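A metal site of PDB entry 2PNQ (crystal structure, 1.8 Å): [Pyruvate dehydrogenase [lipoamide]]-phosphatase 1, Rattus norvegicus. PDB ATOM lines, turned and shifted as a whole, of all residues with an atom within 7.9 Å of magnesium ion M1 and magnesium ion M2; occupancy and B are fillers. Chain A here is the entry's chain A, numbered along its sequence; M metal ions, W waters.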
ATOM      1  N   ASN A  49       4.662  20.595 -17.816  1.00  0.00           N
ATOM      2  CA  ASN A  49       3.979  20.723 -19.097  1.00  0.00           C
ATOM      3  C   ASN A  49       4.141  19.444 -19.914  1.00  0.00           C
ATOM      4  O   ASN A  49       5.097  18.713 -19.689  1.00  0.00           O
ATOM      5  CB  ASN A  49       4.542  21.908 -19.871  1.00  0.00           C
ATOM      6  CG  ASN A  49       4.349  23.231 -19.151  1.00  0.00           C
ATOM      7  OD1 ASN A  49       5.171  23.630 -18.333  1.00  0.00           O
ATOM      8  ND2 ASN A  49       3.241  23.924 -19.450  1.00  0.00           N
ATOM      9  N   ILE A  52       7.837  18.851 -21.741  1.00  0.00           N
ATOM     10  CA  ILE A  52       8.415  19.868 -20.878  1.00  0.00           C
ATOM     11  C   ILE A  52       8.955  21.035 -21.744  1.00  0.00           C
ATOM     12  O   ILE A  52       9.400  20.808 -22.881  1.00  0.00           O
ATOM     13  CB  ILE A  52       9.519  19.219 -20.017  1.00  0.00           C
ATOM     14  CG1 ILE A  52       9.897  20.122 -18.837  1.00  0.00           C
ATOM     15  CG2 ILE A  52      10.687  18.895 -20.897  1.00  0.00           C
ATOM     16  CD1 ILE A  52      11.002  19.560 -17.954  1.00  0.00           C
ATOM     17  N   GLU A  53       8.924  22.264 -21.235  1.00  0.00           N
ATOM     18  CA  GLU A  53       9.373  23.411 -22.035  1.00  0.00           C
ATOM     19  C   GLU A  53      10.779  23.866 -21.655  1.00  0.00           C
ATOM     20  O   GLU A  53      11.400  24.628 -22.383  1.00  0.00           O
ATOM     21  CB  GLU A  53       8.363  24.535 -21.871  1.00  0.00           C
ATOM     22  CG  GLU A  53       6.943  24.038 -22.067  1.00  0.00           C
ATOM     23  CD  GLU A  53       5.944  25.161 -22.264  1.00  0.00           C
ATOM     24  OE1 GLU A  53       5.840  26.029 -21.370  1.00  0.00           O
ATOM     25  OE2 GLU A  53       5.263  25.184 -23.308  1.00  0.00           O
ATOM     26  N   ASP A  54      11.258  23.374 -20.515  1.00  0.00           N
ATOM     27  CA  ASP A  54      12.600  23.648 -19.993  1.00  0.00           C
ATOM     28  C   ASP A  54      13.638  22.690 -20.637  1.00  0.00           C
ATOM     29  O   ASP A  54      13.368  21.497 -20.825  1.00  0.00           O
ATOM     30  CB  ASP A  54      12.656  23.355 -18.495  1.00  0.00           C
ATOM     31  CG  ASP A  54      12.357  24.534 -17.618  1.00  0.00           C
ATOM     32  OD1 ASP A  54      11.877  25.595 -18.114  1.00  0.00           O
ATOM     33  OD2 ASP A  54      12.612  24.367 -16.407  1.00  0.00           O
ATOM     34  N   ARG A  55      14.835  23.208 -20.952  1.00  0.00           N
ATOM     35  CA  ARG A  55      15.899  22.354 -21.458  1.00  0.00           C
ATOM     36  C   ARG A  55      17.163  22.620 -20.665  1.00  0.00           C
ATOM     37  O   ARG A  55      17.299  23.666 -20.042  1.00  0.00           O
ATOM     38  CB  ARG A  55      16.127  22.584 -22.953  1.00  0.00           C
ATOM     39  CG  ARG A  55      15.324  21.636 -23.914  1.00  0.00           C
ATOM     40  CD  ARG A  55      13.885  21.394 -23.436  1.00  0.00           C
ATOM     41  NE  ARG A  55      12.860  21.172 -24.457  1.00  0.00           N
ATOM     42  CZ  ARG A  55      12.909  20.217 -25.369  1.00  0.00           C
ATOM     43  NH1 ARG A  55      13.953  19.404 -25.397  1.00  0.00           N
ATOM     44  NH2 ARG A  55      11.911  20.071 -26.241  1.00  0.00           N
ATOM     45  N   PHE A  72      17.565  26.419 -19.996  1.00  0.00           N
ATOM     46  CA  PHE A  72      16.711  27.218 -20.862  1.00  0.00           C
ATOM     47  C   PHE A  72      15.240  26.983 -20.569  1.00  0.00           C
ATOM     48  O   PHE A  72      14.728  25.875 -20.663  1.00  0.00           O
ATOM     49  CB  PHE A  72      16.997  26.876 -22.328  1.00  0.00           C
ATOM     50  CG  PHE A  72      18.461  26.880 -22.678  1.00  0.00           C
ATOM     51  CD1 PHE A  72      19.302  25.817 -22.300  1.00  0.00           C
ATOM     52  CD2 PHE A  72      19.013  27.939 -23.415  1.00  0.00           C
ATOM     53  CE1 PHE A  72      20.665  25.802 -22.656  1.00  0.00           C
ATOM     54  CE2 PHE A  72      20.375  27.943 -23.779  1.00  0.00           C
ATOM     55  CZ  PHE A  72      21.207  26.878 -23.404  1.00  0.00           C
ATOM     56  N   ASP A  73      14.579  28.076 -20.209  1.00  0.00           N
ATOM     57  CA  ASP A  73      13.184  28.031 -19.886  1.00  0.00           C
ATOM     58  C   ASP A  73      12.325  28.407 -21.105  1.00  0.00           C
ATOM     59  O   ASP A  73      12.261  29.567 -21.492  1.00  0.00           O
ATOM     60  CB  ASP A  73      12.916  28.991 -18.736  1.00  0.00           C
ATOM     61  CG  ASP A  73      11.518  28.907 -18.273  1.00  0.00           C
ATOM     62  OD1 ASP A  73      10.732  28.339 -19.009  1.00  0.00           O
ATOM     63  OD2 ASP A  73      11.098  29.365 -17.211  1.00  0.00           O
ATOM     64  N   GLY A  74      11.674  27.422 -21.734  1.00  0.00           N
ATOM     65  CA  GLY A  74      10.881  27.758 -22.901  1.00  0.00           C
ATOM     66  C   GLY A  74       9.447  28.128 -22.546  1.00  0.00           C
ATOM     67  O   GLY A  74       8.971  27.871 -21.416  1.00  0.00           O
ATOM     68  N   HIS A  75       8.772  28.789 -23.474  1.00  0.00           N
ATOM     69  CA  HIS A  75       7.373  29.100 -23.311  1.00  0.00           C
ATOM     70  C   HIS A  75       6.678  29.132 -24.637  1.00  0.00           C
ATOM     71  O   HIS A  75       7.343  29.296 -25.672  1.00  0.00           O
ATOM     72  CB  HIS A  75       7.130  30.416 -22.526  1.00  0.00           C
ATOM     73  CG  HIS A  75       7.873  31.618 -23.025  1.00  0.00           C
ATOM     74  ND1 HIS A  75       7.419  32.406 -24.062  1.00  0.00           N
ATOM     75  CD2 HIS A  75       8.977  32.236 -22.538  1.00  0.00           C
ATOM     76  CE1 HIS A  75       8.206  33.455 -24.186  1.00  0.00           C
ATOM     77  NE2 HIS A  75       9.156  33.377 -23.273  1.00  0.00           N
ATOM     78  N   ALA A  76       5.369  28.956 -24.605  1.00  0.00           N
ATOM     79  CA  ALA A  76       4.585  28.881 -25.816  1.00  0.00           C
ATOM     80  C   ALA A  76       5.050  27.689 -26.640  1.00  0.00           C
ATOM     81  O   ALA A  76       4.925  27.662 -27.860  1.00  0.00           O
ATOM     82  CB  ALA A  76       4.722  30.168 -26.639  1.00  0.00           C
ATOM     83  N   GLY A  77       5.605  26.706 -25.943  1.00  0.00           N
ATOM     84  CA  GLY A  77       6.119  25.517 -26.613  1.00  0.00           C
ATOM     85  C   GLY A  77       7.552  25.199 -26.237  1.00  0.00           C
ATOM     86  O   GLY A  77       8.161  25.929 -25.461  1.00  0.00           O
ATOM     87  N   SER A  81      13.192  26.714 -26.983  1.00  0.00           N
ATOM     88  CA  SER A  81      14.101  26.268 -25.934  1.00  0.00           C
ATOM     89  C   SER A  81      14.923  25.067 -26.385  1.00  0.00           C
ATOM     90  O   SER A  81      16.085  24.955 -26.032  1.00  0.00           O
ATOM     91  CB  SER A  81      13.326  25.937 -24.641  1.00  0.00           C
ATOM     92  OG  SER A  81      12.188  25.140 -24.908  1.00  0.00           O
ATOM     93  N   GLY A 200       9.315  30.870 -27.521  1.00  0.00           N
ATOM     94  CA  GLY A 200      10.365  31.683 -26.928  1.00  0.00           C
ATOM     95  C   GLY A 200      11.153  30.929 -25.898  1.00  0.00           C
ATOM     96  O   GLY A 200      10.759  29.831 -25.498  1.00  0.00           O
ATOM     97  N   ALA A 201      12.280  31.485 -25.456  1.00  0.00           N
ATOM     98  CA  ALA A 201      13.066  30.796 -24.454  1.00  0.00           C
ATOM     99  C   ALA A 201      14.063  31.700 -23.770  1.00  0.00           C
ATOM    100  O   ALA A 201      14.683  32.607 -24.363  1.00  0.00           O
ATOM    101  CB  ALA A 201      13.811  29.620 -25.092  1.00  0.00           C
ATOM    102  N   THR A 202      14.168  31.425 -22.489  1.00  0.00           N
ATOM    103  CA  THR A 202      15.107  32.042 -21.582  1.00  0.00           C
ATOM    104  C   THR A 202      16.457  31.354 -21.755  1.00  0.00           C
ATOM    105  O   THR A 202      16.515  30.293 -22.382  1.00  0.00           O
ATOM    106  CB  THR A 202      14.591  31.843 -20.135  1.00  0.00           C
ATOM    107  OG1 THR A 202      13.635  32.862 -19.841  1.00  0.00           O
ATOM    108  CG2 THR A 202      15.692  31.916 -19.139  1.00  0.00           C
ATOM    109  N   ASP A 220      14.443  35.149 -16.897  1.00  0.00           N
ATOM    110  CA  ASP A 220      14.188  34.989 -15.463  1.00  0.00           C
ATOM    111  C   ASP A 220      14.730  33.672 -14.885  1.00  0.00           C
ATOM    112  O   ASP A 220      14.352  33.293 -13.771  1.00  0.00           O
ATOM    113  CB  ASP A 220      12.693  35.145 -15.169  1.00  0.00           C
ATOM    114  CG  ASP A 220      11.799  34.291 -16.053  1.00  0.00           C
ATOM    115  OD1 ASP A 220      10.575  34.586 -16.048  1.00  0.00           O
ATOM    116  OD2 ASP A 220      12.281  33.360 -16.727  1.00  0.00           O
ATOM    117  N   SER A 221      15.573  32.960 -15.620  1.00  0.00           N
ATOM    118  CA  SER A 221      16.237  31.831 -14.995  1.00  0.00           C
ATOM    119  C   SER A 221      17.398  32.400 -14.170  1.00  0.00           C
ATOM    120  O   SER A 221      17.646  33.606 -14.279  1.00  0.00           O
ATOM    121  CB  SER A 221      16.760  30.855 -16.034  1.00  0.00           C
ATOM    122  OG  SER A 221      15.677  30.272 -16.723  1.00  0.00           O
ATOM    123  N   PRO A 278       9.119  37.261 -18.623  1.00  0.00           N
ATOM    124  CA  PRO A 278      10.544  37.570 -18.839  1.00  0.00           C
ATOM    125  C   PRO A 278      10.686  38.783 -19.709  1.00  0.00           C
ATOM    126  O   PRO A 278       9.927  38.920 -20.656  1.00  0.00           O
ATOM    127  CB  PRO A 278      11.099  36.317 -19.536  1.00  0.00           C
ATOM    128  CG  PRO A 278      10.036  35.286 -19.417  1.00  0.00           C
ATOM    129  CD  PRO A 278       8.739  36.038 -19.353  1.00  0.00           C
ATOM    130  N   ALA A 345      19.410  27.274 -12.574  1.00  0.00           N
ATOM    131  CA  ALA A 345      18.062  26.695 -12.538  1.00  0.00           C
ATOM    132  C   ALA A 345      17.055  27.645 -13.112  1.00  0.00           C
ATOM    133  O   ALA A 345      17.289  28.853 -13.137  1.00  0.00           O
ATOM    134  CB  ALA A 345      17.669  26.364 -11.108  1.00  0.00           C
ATOM    135  N   THR A 346      15.946  27.098 -13.585  1.00  0.00           N
ATOM    136  CA  THR A 346      14.892  27.954 -14.092  1.00  0.00           C
ATOM    137  C   THR A 346      14.045  28.448 -12.926  1.00  0.00           C
ATOM    138  O   THR A 346      14.194  27.952 -11.812  1.00  0.00           O
ATOM    139  CB  THR A 346      14.022  27.229 -15.135  1.00  0.00           C
ATOM    140  OG1 THR A 346      13.550  25.975 -14.631  1.00  0.00           O
ATOM    141  CG2 THR A 346      14.842  26.998 -16.397  1.00  0.00           C
ATOM    142  N   ASP A 347      13.161  29.421 -13.179  1.00  0.00           N
ATOM    143  CA  ASP A 347      12.315  29.983 -12.131  1.00  0.00           C
ATOM    144  C   ASP A 347      11.426  28.917 -11.501  1.00  0.00           C
ATOM    145  O   ASP A 347      10.728  29.173 -10.525  1.00  0.00           O
ATOM    146  CB  ASP A 347      11.451  31.073 -12.699  1.00  0.00           C
ATOM    147  CG  ASP A 347      10.473  30.544 -13.703  1.00  0.00           C
ATOM    148  OD1 ASP A 347      10.799  29.456 -14.220  1.00  0.00           O
ATOM    149  OD2 ASP A 347       9.468  31.213 -13.943  1.00  0.00           O
ATOM    150  N   GLY A 348      11.452  27.722 -12.084  1.00  0.00           N
ATOM    151  CA  GLY A 348      10.705  26.655 -11.470  1.00  0.00           C
ATOM    152  C   GLY A 348      11.183  26.370 -10.051  1.00  0.00           C
ATOM    153  O   GLY A 348      10.440  25.970  -9.152  1.00  0.00           O
ATOM    154  N   LEU A 349      12.468  26.588  -9.880  1.00  0.00           N
ATOM    155  CA  LEU A 349      13.121  26.400  -8.608  1.00  0.00           C
ATOM    156  C   LEU A 349      12.963  27.621  -7.697  1.00  0.00           C
ATOM    157  O   LEU A 349      12.420  27.509  -6.604  1.00  0.00           O
ATOM    158  CB  LEU A 349      14.619  26.141  -8.814  1.00  0.00           C
ATOM    159  CG  LEU A 349      15.550  26.178  -7.579  1.00  0.00           C
ATOM    160  CD1 LEU A 349      15.151  25.091  -6.592  1.00  0.00           C
ATOM    161  CD2 LEU A 349      16.983  25.979  -7.993  1.00  0.00           C
ATOM    162  N   GLU A 351      10.958  29.939  -7.461  1.00  0.00           N
ATOM    163  CA  GLU A 351       9.622  30.347  -7.030  1.00  0.00           C
ATOM    164  C   GLU A 351       9.199  29.586  -5.787  1.00  0.00           C
ATOM    165  O   GLU A 351       8.200  29.937  -5.141  1.00  0.00           O
ATOM    166  CB  GLU A 351       8.582  30.083  -8.120  1.00  0.00           C
ATOM    167  CG  GLU A 351       8.596  31.057  -9.279  1.00  0.00           C
ATOM    168  CD  GLU A 351       8.177  32.461  -8.880  1.00  0.00           C
ATOM    169  OE1 GLU A 351       7.199  32.587  -8.100  1.00  0.00           O
ATOM    170  OE2 GLU A 351       8.819  33.439  -9.335  1.00  0.00           O
ATOM    171  N   ARG A 444       4.093  24.112  -9.615  1.00  0.00           N
ATOM    172  CA  ARG A 444       3.371  24.776 -10.709  1.00  0.00           C
ATOM    173  C   ARG A 444       4.207  25.205 -11.906  1.00  0.00           C
ATOM    174  O   ARG A 444       3.745  26.048 -12.660  1.00  0.00           O
ATOM    175  CB  ARG A 444       2.611  25.965 -10.140  1.00  0.00           C
ATOM    176  CG  ARG A 444       1.305  25.527  -9.498  1.00  0.00           C
ATOM    177  CD  ARG A 444       0.726  26.639  -8.671  1.00  0.00           C
ATOM    178  NE  ARG A 444      -0.597  27.043  -9.112  1.00  0.00           N
ATOM    179  CZ  ARG A 444      -0.887  27.450 -10.343  1.00  0.00           C
ATOM    180  NH1 ARG A 444       0.056  27.493 -11.284  1.00  0.00           N
ATOM    181  NH2 ARG A 444      -2.123  27.788 -10.644  1.00  0.00           N
ATOM    182  N   ASP A 445       5.391  24.633 -12.120  1.00  0.00           N
ATOM    183  CA  ASP A 445       6.179  24.982 -13.323  1.00  0.00           C
ATOM    184  C   ASP A 445       7.276  23.950 -13.585  1.00  0.00           C
ATOM    185  O   ASP A 445       7.694  23.234 -12.682  1.00  0.00           O
ATOM    186  CB  ASP A 445       6.817  26.370 -13.173  1.00  0.00           C
ATOM    187  CG  ASP A 445       7.521  26.847 -14.449  1.00  0.00           C
ATOM    188  OD1 ASP A 445       7.203  26.311 -15.541  1.00  0.00           O
ATOM    189  OD2 ASP A 445       8.379  27.771 -14.313  1.00  0.00           O
ATOM    190  N   ASP A 446       7.730  23.852 -14.828  1.00  0.00           N
ATOM    191  CA  ASP A 446       8.825  22.953 -15.087  1.00  0.00           C
ATOM    192  C   ASP A 446       9.982  23.331 -14.174  1.00  0.00           C
ATOM    193  O   ASP A 446      10.171  24.518 -13.887  1.00  0.00           O
ATOM    194  CB  ASP A 446       9.274  23.067 -16.546  1.00  0.00           C
ATOM    195  CG  ASP A 446       8.130  22.903 -17.520  1.00  0.00           C
ATOM    196  OD1 ASP A 446       7.136  22.251 -17.133  1.00  0.00           O
ATOM    197  OD2 ASP A 446       8.220  23.417 -18.669  1.00  0.00           O
ATOM    198  N   ILE A 447      10.752  22.356 -13.710  1.00  0.00           N
ATOM    199  CA  ILE A 447      11.871  22.624 -12.821  1.00  0.00           C
ATOM    200  C   ILE A 447      13.115  21.953 -13.326  1.00  0.00           C
ATOM    201  O   ILE A 447      13.165  20.727 -13.397  1.00  0.00           O
ATOM    202  CB  ILE A 447      11.623  22.082 -11.365  1.00  0.00           C
ATOM    203  CG1 ILE A 447      10.624  22.970 -10.633  1.00  0.00           C
ATOM    204  CG2 ILE A 447      12.910  22.088 -10.571  1.00  0.00           C
ATOM    205  CD1 ILE A 447      10.196  22.428  -9.287  1.00  0.00           C
ATOM    206  N   THR A 448      14.114  22.742 -13.699  1.00  0.00           N
ATOM    207  CA  THR A 448      15.365  22.146 -14.130  1.00  0.00           C
ATOM    208  C   THR A 448      16.529  22.778 -13.387  1.00  0.00           C
ATOM    209  O   THR A 448      16.585  24.000 -13.208  1.00  0.00           O
ATOM    210  CB  THR A 448      15.562  22.299 -15.650  1.00  0.00           C
ATOM    211  OG1 THR A 448      15.642  23.678 -15.972  1.00  0.00           O
ATOM    212  CG2 THR A 448      14.395  21.744 -16.392  1.00  0.00           C
HETATM  213 MG    MG M   1       9.713  28.561 -15.763  1.00  0.00          MG
HETATM  214 MG    MG M   2       8.721  27.869 -19.259  1.00  0.00          MG
HETATM  215  O   HOH W   1      10.894  26.742 -15.635  1.00  0.00           O
HETATM  216  O   HOH W   2       8.530  30.375 -15.877  1.00  0.00           O
HETATM  217  O   HOH W   3       8.461  27.751 -17.217  1.00  0.00           O
HETATM  218  O   HOH W   4       9.233  25.761 -19.278  1.00  0.00           O
HETATM  219  O   HOH W   5       6.674  27.251 -19.518  1.00  0.00           O
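O of Asp 73 sits at hydrogen-bond distance from N of Thr 202. O of Glu 53 is in hydrogen-bond range of N of Gly 74 (2.9 Å).
Along chain A the residues within 4 Å of magnesium ion M1 span positions 73 to 445.
Within 4 Å of magnesium ion M2: Asp 73 and Gly 74. The nearest printed residue that does not touch magnesium ion M2 is Glu 53 (4.02 Å).
Magnesium ion M1 is bound by water W3, the side-chain carboxylate of Asp 347, the side-chain carboxylate of Asp 445, the side-chain carboxylate of Asp 73, water W2 and water W1. Magnesium ion M1 has six donor atoms within binding distance.
Magnesium ion M2 is bound by water W3 (2.1 Å), the side-chain carboxylate (OD1) of Asp 73 (2.1 Å), water W5 (2.2 Å), water W4 (2.2 Å) and the backbone carbonyl oxygen (O) of Gly 74 (2.2 Å).
Water W1 lies within hydrogen-bond range of OD1 of Asp 54, O of Asp 446 and OG1 of Thr 346. Water W4 bridges the side-chain carboxylate (OD2) of Asp 446 and the side-chain carboxylate (OD1) of Asp 54.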
